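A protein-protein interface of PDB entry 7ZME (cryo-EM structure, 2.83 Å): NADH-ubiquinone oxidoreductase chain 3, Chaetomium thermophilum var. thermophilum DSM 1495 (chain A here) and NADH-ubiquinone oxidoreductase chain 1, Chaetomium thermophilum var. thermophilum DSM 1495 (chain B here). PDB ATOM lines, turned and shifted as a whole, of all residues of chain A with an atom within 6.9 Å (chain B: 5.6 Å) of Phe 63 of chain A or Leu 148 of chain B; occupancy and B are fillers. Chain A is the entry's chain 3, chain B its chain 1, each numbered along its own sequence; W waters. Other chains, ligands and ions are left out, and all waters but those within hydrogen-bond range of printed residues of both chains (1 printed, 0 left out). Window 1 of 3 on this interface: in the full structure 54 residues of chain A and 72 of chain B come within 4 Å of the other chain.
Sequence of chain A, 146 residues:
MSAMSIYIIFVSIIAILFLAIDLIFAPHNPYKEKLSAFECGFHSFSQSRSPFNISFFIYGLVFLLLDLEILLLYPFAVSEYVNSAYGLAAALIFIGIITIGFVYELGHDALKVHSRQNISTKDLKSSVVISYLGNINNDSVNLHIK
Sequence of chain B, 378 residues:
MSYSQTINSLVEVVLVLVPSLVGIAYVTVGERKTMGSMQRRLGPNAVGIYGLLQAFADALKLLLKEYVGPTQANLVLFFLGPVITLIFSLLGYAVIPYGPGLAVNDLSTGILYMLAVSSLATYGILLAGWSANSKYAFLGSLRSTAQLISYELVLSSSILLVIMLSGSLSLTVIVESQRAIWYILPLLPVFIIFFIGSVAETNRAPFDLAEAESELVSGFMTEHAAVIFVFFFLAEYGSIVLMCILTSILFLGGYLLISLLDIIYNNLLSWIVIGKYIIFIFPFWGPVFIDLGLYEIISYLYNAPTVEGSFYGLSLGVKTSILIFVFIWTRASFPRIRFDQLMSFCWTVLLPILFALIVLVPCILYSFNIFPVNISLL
Water W1 bridges the side-chain carboxylate of Glu 152 of chain B (2.8 Å) and the side-chain carboxylate of Asp 67 of chain A (2.9 Å).
Of the printed residues of chain B, Gly 60 of chain A touches Ile 149.
Printed residues of chain B within 4 Å of Val 62 of chain A: Trp 347 (3.7 Å).
Of the printed residues of chain B, Asp 67 of chain A touches Glu 152.
Leu 148 of chain B touches just one residue of chain A: Phe 63.
Of the printed residues of chain A, Ile 149 of chain B touches Tyr 59, Gly 60 and Phe 63.
Tyr 151 of chain B touches none of the printed residues of chain A.
The nearest printed residue of chain A that does not touch Leu 148 of chain B is Asp 67 of chain A (7.0 Å).
The nearest printed residue of chain B that does not touch Asp 67 of chain A is Leu 153 of chain B (4.5 Å).
Hydrophobic or aromatic side chains of chain B within 4 Å of the printed part of chain A: Leu 148, Ile 149, Leu 153 and Trp 347.
Hydrophobic or aromatic side chains of chain A that line the printed part of chain B: Tyr 59, Val 62, Phe 63 and Leu 66.
Among the printed residues, no Asp or Glu carboxylate lies within 4 Å of a Lys or Arg side-chain nitrogen of the other chain.
Among the printed residues, merely in contact across the chains: Phe 63 of chain A with Leu 153 of chain B (3.2 Å), Leu 66 of chain A with Leu 153 of chain B (3.3 Å), Tyr 59 of chain A with Trp 347 of chain B (3.3 Å), Leu 66 of chain A with Trp 347 of chain B (3.4 Å), Phe 63 of chain A with Glu 152 of chain B (3.5 Å), Tyr 59 of chain A with Ile 149 of chain B (3.5 Å), Asp 67 of chain A with Glu 152 of chain B (3.5 Å), Phe 63 of chain A with Ile 149 of chain B (3.7 Å), Val 62 of chain A with Trp 347 of chain B (3.7 Å), Gly 60 of chain A with Ile 149 of chain B (3.9 Å) and Phe 63 of chain A with Leu 148 of chain B (3.9 Å).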
ATOM      1  N   ILE A  58     -35.496  28.779 -24.618  1.00  0.00           N
ATOM      2  CA  ILE A  58     -35.280  27.658 -25.576  1.00  0.00           C
ATOM      3  C   ILE A  58     -33.767  27.453 -25.728  1.00  0.00           C
ATOM      4  O   ILE A  58     -33.351  26.318 -25.997  1.00  0.00           O
ATOM      5  CB  ILE A  58     -36.043  27.932 -26.892  1.00  0.00           C
ATOM      6  CG1 ILE A  58     -37.544  28.091 -26.645  1.00  0.00           C
ATOM      7  CG2 ILE A  58     -35.761  26.873 -27.942  1.00  0.00           C
ATOM      8  CD1 ILE A  58     -38.350  28.341 -27.894  1.00  0.00           C
ATOM      9  N   TYR A  59     -32.978  28.490 -25.444  1.00  0.00           N
ATOM     10  CA  TYR A  59     -31.498  28.399 -25.513  1.00  0.00           C
ATOM     11  C   TYR A  59     -31.010  27.696 -24.244  1.00  0.00           C
ATOM     12  O   TYR A  59     -30.032  26.952 -24.330  1.00  0.00           O
ATOM     13  CB  TYR A  59     -30.872  29.795 -25.472  1.00  0.00           C
ATOM     14  CG  TYR A  59     -30.730  30.568 -26.757  1.00  0.00           C
ATOM     15  CD1 TYR A  59     -31.760  31.352 -27.246  1.00  0.00           C
ATOM     16  CD2 TYR A  59     -29.529  30.583 -27.438  1.00  0.00           C
ATOM     17  CE1 TYR A  59     -31.614  32.091 -28.408  1.00  0.00           C
ATOM     18  CE2 TYR A  59     -29.365  31.315 -28.599  1.00  0.00           C
ATOM     19  CZ  TYR A  59     -30.410  32.073 -29.087  1.00  0.00           C
ATOM     20  OH  TYR A  59     -30.241  32.791 -30.235  1.00  0.00           O
ATOM     21  N   GLY A  60     -31.654  27.943 -23.102  1.00  0.00           N
ATOM     22  CA  GLY A  60     -31.286  27.196 -21.913  1.00  0.00           C
ATOM     23  C   GLY A  60     -31.625  25.722 -22.016  1.00  0.00           C
ATOM     24  O   GLY A  60     -30.881  24.870 -21.529  1.00  0.00           O
ATOM     25  N   LEU A  61     -32.763  25.389 -22.616  1.00  0.00           N
ATOM     26  CA  LEU A  61     -33.130  23.964 -22.802  1.00  0.00           C
ATOM     27  C   LEU A  61     -32.067  23.264 -23.655  1.00  0.00           C
ATOM     28  O   LEU A  61     -31.667  22.158 -23.277  1.00  0.00           O
ATOM     29  CB  LEU A  61     -34.518  23.892 -23.442  1.00  0.00           C
ATOM     30  CG  LEU A  61     -35.690  24.257 -22.534  1.00  0.00           C
ATOM     31  CD1 LEU A  61     -36.982  24.352 -23.331  1.00  0.00           C
ATOM     32  CD2 LEU A  61     -35.833  23.245 -21.411  1.00  0.00           C
ATOM     33  N   VAL A  62     -31.656  23.867 -24.773  1.00  0.00           N
ATOM     34  CA  VAL A  62     -30.640  23.278 -25.698  1.00  0.00           C
ATOM     35  C   VAL A  62     -29.257  23.213 -25.041  1.00  0.00           C
ATOM     36  O   VAL A  62     -28.548  22.231 -25.283  1.00  0.00           O
ATOM     37  CB  VAL A  62     -30.621  24.003 -27.057  1.00  0.00           C
ATOM     38  CG1 VAL A  62     -31.925  23.821 -27.816  1.00  0.00           C
ATOM     39  CG2 VAL A  62     -30.282  25.478 -26.911  1.00  0.00           C
ATOM     40  N   PHE A  63     -28.890  24.219 -24.247  1.00  0.00           N
ATOM     41  CA  PHE A  63     -27.560  24.284 -23.589  1.00  0.00           C
ATOM     42  C   PHE A  63     -27.377  23.075 -22.678  1.00  0.00           C
ATOM     43  O   PHE A  63     -26.267  22.545 -22.637  1.00  0.00           O
ATOM     44  CB  PHE A  63     -27.440  25.600 -22.815  1.00  0.00           C
ATOM     45  CG  PHE A  63     -26.651  25.565 -21.530  1.00  0.00           C
ATOM     46  CD1 PHE A  63     -25.286  25.781 -21.531  1.00  0.00           C
ATOM     47  CD2 PHE A  63     -27.278  25.359 -20.314  1.00  0.00           C
ATOM     48  CE1 PHE A  63     -24.557  25.744 -20.356  1.00  0.00           C
ATOM     49  CE2 PHE A  63     -26.548  25.320 -19.139  1.00  0.00           C
ATOM     50  CZ  PHE A  63     -25.189  25.516 -19.160  1.00  0.00           C
ATOM     51  N   LEU A  64     -28.436  22.667 -21.981  1.00  0.00           N
ATOM     52  CA  LEU A  64     -28.346  21.532 -21.036  1.00  0.00           C
ATOM     53  C   LEU A  64     -27.960  20.264 -21.791  1.00  0.00           C
ATOM     54  O   LEU A  64     -27.035  19.579 -21.340  1.00  0.00           O
ATOM     55  CB  LEU A  64     -29.734  21.343 -20.416  1.00  0.00           C
ATOM     56  CG  LEU A  64     -30.196  22.432 -19.455  1.00  0.00           C
ATOM     57  CD1 LEU A  64     -31.530  22.059 -18.834  1.00  0.00           C
ATOM     58  CD2 LEU A  64     -29.152  22.663 -18.380  1.00  0.00           C
ATOM     59  N   LEU A  65     -28.622  19.996 -22.910  1.00  0.00           N
ATOM     60  CA  LEU A  65     -28.360  18.774 -23.700  1.00  0.00           C
ATOM     61  C   LEU A  65     -26.969  18.806 -24.335  1.00  0.00           C
ATOM     62  O   LEU A  65     -26.293  17.778 -24.297  1.00  0.00           O
ATOM     63  CB  LEU A  65     -29.465  18.659 -24.753  1.00  0.00           C
ATOM     64  CG  LEU A  65     -30.886  18.767 -24.204  1.00  0.00           C
ATOM     65  CD1 LEU A  65     -31.887  19.001 -25.321  1.00  0.00           C
ATOM     66  CD2 LEU A  65     -31.251  17.532 -23.395  1.00  0.00           C
ATOM     67  N   LEU A  66     -26.573  19.931 -24.917  1.00  0.00           N
ATOM     68  CA  LEU A  66     -25.251  20.052 -25.577  1.00  0.00           C
ATOM     69  C   LEU A  66     -24.133  19.986 -24.540  1.00  0.00           C
ATOM     70  O   LEU A  66     -23.048  19.498 -24.878  1.00  0.00           O
ATOM     71  CB  LEU A  66     -25.222  21.321 -26.428  1.00  0.00           C
ATOM     72  CG  LEU A  66     -25.411  21.098 -27.927  1.00  0.00           C
ATOM     73  CD1 LEU A  66     -25.718  22.406 -28.639  1.00  0.00           C
ATOM     74  CD2 LEU A  66     -24.184  20.434 -28.529  1.00  0.00           C
ATOM     75  N   ASP A  67     -24.391  20.486 -23.336  1.00  0.00           N
ATOM     76  CA  ASP A  67     -23.408  20.399 -22.232  1.00  0.00           C
ATOM     77  C   ASP A  67     -23.193  18.911 -21.952  1.00  0.00           C
ATOM     78  O   ASP A  67     -22.059  18.519 -21.661  1.00  0.00           O
ATOM     79  CB  ASP A  67     -23.925  21.170 -21.015  1.00  0.00           C
ATOM     80  CG  ASP A  67     -22.889  21.582 -19.983  1.00  0.00           C
ATOM     81  OD1 ASP A  67     -21.740  21.127 -20.082  1.00  0.00           O
ATOM     82  OD2 ASP A  67     -23.248  22.362 -19.081  1.00  0.00           O
ATOM     83  N   LEU A  68     -24.249  18.115 -22.086  1.00  0.00           N
ATOM     84  CA  LEU A  68     -24.141  16.668 -21.773  1.00  0.00           C
ATOM     85  C   LEU A  68     -23.330  16.037 -22.895  1.00  0.00           C
ATOM     86  O   LEU A  68     -22.506  15.156 -22.607  1.00  0.00           O
ATOM     87  CB  LEU A  68     -25.545  16.071 -21.695  1.00  0.00           C
ATOM     88  CG  LEU A  68     -26.381  16.519 -20.498  1.00  0.00           C
ATOM     89  CD1 LEU A  68     -27.843  16.158 -20.692  1.00  0.00           C
ATOM     90  CD2 LEU A  68     -25.846  15.919 -19.211  1.00  0.00           C
ATOM     91  N   GLU A  69     -23.574  16.473 -24.130  1.00  0.00           N
ATOM     92  CA  GLU A  69     -22.897  15.931 -25.336  1.00  0.00           C
ATOM     93  C   GLU A  69     -21.387  16.198 -25.370  1.00  0.00           C
ATOM     94  O   GLU A  69     -20.664  15.294 -25.817  1.00  0.00           O
ATOM     95  CB  GLU A  69     -23.667  16.419 -26.560  1.00  0.00           C
ATOM     96  CG  GLU A  69     -25.051  15.806 -26.640  1.00  0.00           C
ATOM     97  CD  GLU A  69     -26.130  16.626 -27.321  1.00  0.00           C
ATOM     98  OE1 GLU A  69     -27.305  16.212 -27.273  1.00  0.00           O
ATOM     99  OE2 GLU A  69     -25.798  17.671 -27.897  1.00  0.00           O
ATOM    100  N   THR B 122     -19.857  32.311 -11.623  1.00  0.00           N
ATOM    101  CA  THR B 122     -20.925  32.947 -12.386  1.00  0.00           C
ATOM    102  C   THR B 122     -22.254  32.864 -11.647  1.00  0.00           C
ATOM    103  O   THR B 122     -23.052  33.807 -11.683  1.00  0.00           O
ATOM    104  CB  THR B 122     -21.036  32.300 -13.765  1.00  0.00           C
ATOM    105  OG1 THR B 122     -19.733  32.217 -14.357  1.00  0.00           O
ATOM    106  CG2 THR B 122     -21.940  33.117 -14.669  1.00  0.00           C
ATOM    107  N   ARG B 143     -29.135  38.777 -17.725  1.00  0.00           N
ATOM    108  CA  ARG B 143     -28.132  38.911 -18.813  1.00  0.00           C
ATOM    109  C   ARG B 143     -26.948  37.987 -18.541  1.00  0.00           C
ATOM    110  O   ARG B 143     -26.457  37.388 -19.494  1.00  0.00           O
ATOM    111  CB  ARG B 143     -27.737  40.376 -18.992  1.00  0.00           C
ATOM    112  CG  ARG B 143     -28.788  41.210 -19.705  1.00  0.00           C
ATOM    113  CD  ARG B 143     -28.268  42.600 -19.972  1.00  0.00           C
ATOM    114  NE  ARG B 143     -29.132  43.335 -20.876  1.00  0.00           N
ATOM    115  CZ  ARG B 143     -28.830  44.516 -21.393  1.00  0.00           C
ATOM    116  NH1 ARG B 143     -27.677  45.088 -21.093  1.00  0.00           N
ATOM    117  NH2 ARG B 143     -29.676  45.117 -22.210  1.00  0.00           N
ATOM    118  N   SER B 144     -26.527  37.870 -17.283  1.00  0.00           N
ATOM    119  CA  SER B 144     -25.396  36.989 -16.905  1.00  0.00           C
ATOM    120  C   SER B 144     -25.724  35.533 -17.246  1.00  0.00           C
ATOM    121  O   SER B 144     -24.835  34.819 -17.719  1.00  0.00           O
ATOM    122  CB  SER B 144     -25.140  37.148 -15.438  1.00  0.00           C
ATOM    123  OG  SER B 144     -24.556  35.979 -14.887  1.00  0.00           O
ATOM    124  N   THR B 145     -26.975  35.132 -16.991  1.00  0.00           N
ATOM    125  CA  THR B 145     -27.412  33.748 -17.263  1.00  0.00           C
ATOM    126  C   THR B 145     -27.417  33.504 -18.775  1.00  0.00           C
ATOM    127  O   THR B 145     -26.964  32.435 -19.188  1.00  0.00           O
ATOM    128  CB  THR B 145     -28.767  33.511 -16.589  1.00  0.00           C
ATOM    129  OG1 THR B 145     -28.709  34.215 -15.352  1.00  0.00           O
ATOM    130  CG2 THR B 145     -29.064  32.048 -16.347  1.00  0.00           C
ATOM    131  N   ALA B 146     -27.901  34.456 -19.549  1.00  0.00           N
ATOM    132  CA  ALA B 146     -27.918  34.343 -21.023  1.00  0.00           C
ATOM    133  C   ALA B 146     -26.486  34.237 -21.518  1.00  0.00           C
ATOM    134  O   ALA B 146     -26.235  33.422 -22.414  1.00  0.00           O
ATOM    135  CB  ALA B 146     -28.548  35.573 -21.597  1.00  0.00           C
ATOM    136  N   GLN B 147     -25.593  35.040 -20.937  1.00  0.00           N
ATOM    137  CA  GLN B 147     -24.178  35.051 -21.360  1.00  0.00           C
ATOM    138  C   GLN B 147     -23.517  33.695 -21.071  1.00  0.00           C
ATOM    139  O   GLN B 147     -22.798  33.222 -21.945  1.00  0.00           O
ATOM    140  CB  GLN B 147     -23.474  36.277 -20.784  1.00  0.00           C
ATOM    141  CG  GLN B 147     -22.167  36.600 -21.485  1.00  0.00           C
ATOM    142  CD  GLN B 147     -21.790  38.052 -21.354  1.00  0.00           C
ATOM    143  OE1 GLN B 147     -20.683  38.452 -21.689  1.00  0.00           O
ATOM    144  NE2 GLN B 147     -22.721  38.855 -20.870  1.00  0.00           N
ATOM    145  N   LEU B 148     -23.734  33.048 -19.997  1.00  0.00           N
ATOM    146  CA  LEU B 148     -23.106  31.739 -19.684  1.00  0.00           C
ATOM    147  C   LEU B 148     -23.618  30.680 -20.649  1.00  0.00           C
ATOM    148  O   LEU B 148     -22.817  29.857 -21.085  1.00  0.00           O
ATOM    149  CB  LEU B 148     -23.293  31.360 -18.209  1.00  0.00           C
ATOM    150  CG  LEU B 148     -24.572  30.632 -17.793  1.00  0.00           C
ATOM    151  CD1 LEU B 148     -24.380  29.124 -17.813  1.00  0.00           C
ATOM    152  CD2 LEU B 148     -24.994  31.070 -16.401  1.00  0.00           C
ATOM    153  N   ILE B 149     -24.957  30.747 -20.964  1.00  0.00           N
ATOM    154  CA  ILE B 149     -25.485  29.798 -21.980  1.00  0.00           C
ATOM    155  C   ILE B 149     -24.692  30.030 -23.268  1.00  0.00           C
ATOM    156  O   ILE B 149     -24.366  29.041 -23.949  1.00  0.00           O
ATOM    157  CB  ILE B 149     -27.000  30.018 -22.171  1.00  0.00           C
ATOM    158  CG1 ILE B 149     -27.799  29.721 -20.900  1.00  0.00           C
ATOM    159  CG2 ILE B 149     -27.535  29.240 -23.361  1.00  0.00           C
ATOM    160  CD1 ILE B 149     -29.183  30.320 -20.914  1.00  0.00           C
ATOM    161  N   SER B 150     -24.407  31.286 -23.597  1.00  0.00           N
ATOM    162  CA  SER B 150     -23.620  31.633 -24.806  1.00  0.00           C
ATOM    163  C   SER B 150     -22.149  31.202 -24.783  1.00  0.00           C
ATOM    164  O   SER B 150     -21.697  30.669 -25.799  1.00  0.00           O
ATOM    165  CB  SER B 150     -23.694  33.114 -25.042  1.00  0.00           C
ATOM    166  OG  SER B 150     -24.996  33.609 -24.801  1.00  0.00           O
ATOM    167  N   TYR B 151     -21.418  31.407 -23.686  1.00  0.00           N
ATOM    168  CA  TYR B 151     -19.946  31.182 -23.730  1.00  0.00           C
ATOM    169  C   TYR B 151     -19.445  29.892 -23.083  1.00  0.00           C
ATOM    170  O   TYR B 151     -18.251  29.610 -23.254  1.00  0.00           O
ATOM    171  CB  TYR B 151     -19.211  32.380 -23.117  1.00  0.00           C
ATOM    172  CG  TYR B 151     -19.443  32.621 -21.643  1.00  0.00           C
ATOM    173  CD1 TYR B 151     -19.048  31.707 -20.682  1.00  0.00           C
ATOM    174  CD2 TYR B 151     -20.024  33.795 -21.200  1.00  0.00           C
ATOM    175  CE1 TYR B 151     -19.272  31.921 -19.334  1.00  0.00           C
ATOM    176  CE2 TYR B 151     -20.246  34.034 -19.855  1.00  0.00           C
ATOM    177  CZ  TYR B 151     -19.863  33.096 -18.917  1.00  0.00           C
ATOM    178  OH  TYR B 151     -20.073  33.326 -17.590  1.00  0.00           O
ATOM    179  N   GLU B 152     -20.298  29.115 -22.423  1.00  0.00           N
ATOM    180  CA  GLU B 152     -19.768  27.957 -21.658  1.00  0.00           C
ATOM    181  C   GLU B 152     -19.470  26.838 -22.645  1.00  0.00           C
ATOM    182  O   GLU B 152     -18.375  26.263 -22.567  1.00  0.00           O
ATOM    183  CB  GLU B 152     -20.797  27.512 -20.615  1.00  0.00           C
ATOM    184  CG  GLU B 152     -20.265  26.527 -19.591  1.00  0.00           C
ATOM    185  CD  GLU B 152     -20.620  25.069 -19.836  1.00  0.00           C
ATOM    186  OE1 GLU B 152     -21.268  24.783 -20.858  1.00  0.00           O
ATOM    187  OE2 GLU B 152     -20.247  24.224 -19.000  1.00  0.00           O
ATOM    188  N   LEU B 153     -20.405  26.563 -23.546  1.00  0.00           N
ATOM    189  CA  LEU B 153     -20.127  25.574 -24.580  1.00  0.00           C
ATOM    190  C   LEU B 153     -18.978  26.014 -25.466  1.00  0.00           C
ATOM    191  O   LEU B 153     -18.163  25.189 -25.886  1.00  0.00           O
ATOM    192  CB  LEU B 153     -21.371  25.309 -25.425  1.00  0.00           C
ATOM    193  CG  LEU B 153     -22.420  24.338 -24.895  1.00  0.00           C
ATOM    194  CD1 LEU B 153     -23.117  24.909 -23.714  1.00  0.00           C
ATOM    195  CD2 LEU B 153     -23.415  24.045 -25.986  1.00  0.00           C
ATOM    196  N   TRP B 347     -24.115  30.930 -31.003  1.00  0.00           N
ATOM    197  CA  TRP B 347     -24.897  29.734 -31.273  1.00  0.00           C
ATOM    198  C   TRP B 347     -25.051  29.431 -32.756  1.00  0.00           C
ATOM    199  O   TRP B 347     -25.274  28.269 -33.111  1.00  0.00           O
ATOM    200  CB  TRP B 347     -26.268  29.887 -30.614  1.00  0.00           C
ATOM    201  CG  TRP B 347     -26.299  29.376 -29.210  1.00  0.00           C
ATOM    202  CD1 TRP B 347     -26.293  30.122 -28.071  1.00  0.00           C
ATOM    203  CD2 TRP B 347     -26.428  28.018 -28.794  1.00  0.00           C
ATOM    204  NE1 TRP B 347     -26.358  29.312 -26.972  1.00  0.00           N
ATOM    205  CE2 TRP B 347     -26.450  28.013 -27.388  1.00  0.00           C
ATOM    206  CE3 TRP B 347     -26.512  26.803 -29.473  1.00  0.00           C
ATOM    207  CZ2 TRP B 347     -26.551  26.842 -26.649  1.00  0.00           C
ATOM    208  CZ3 TRP B 347     -26.613  25.648 -28.742  1.00  0.00           C
ATOM    209  CH2 TRP B 347     -26.629  25.671 -27.342  1.00  0.00           C
HETATM  210  O   HOH W   1     -20.792  22.529 -22.400  1.00  0.00           O
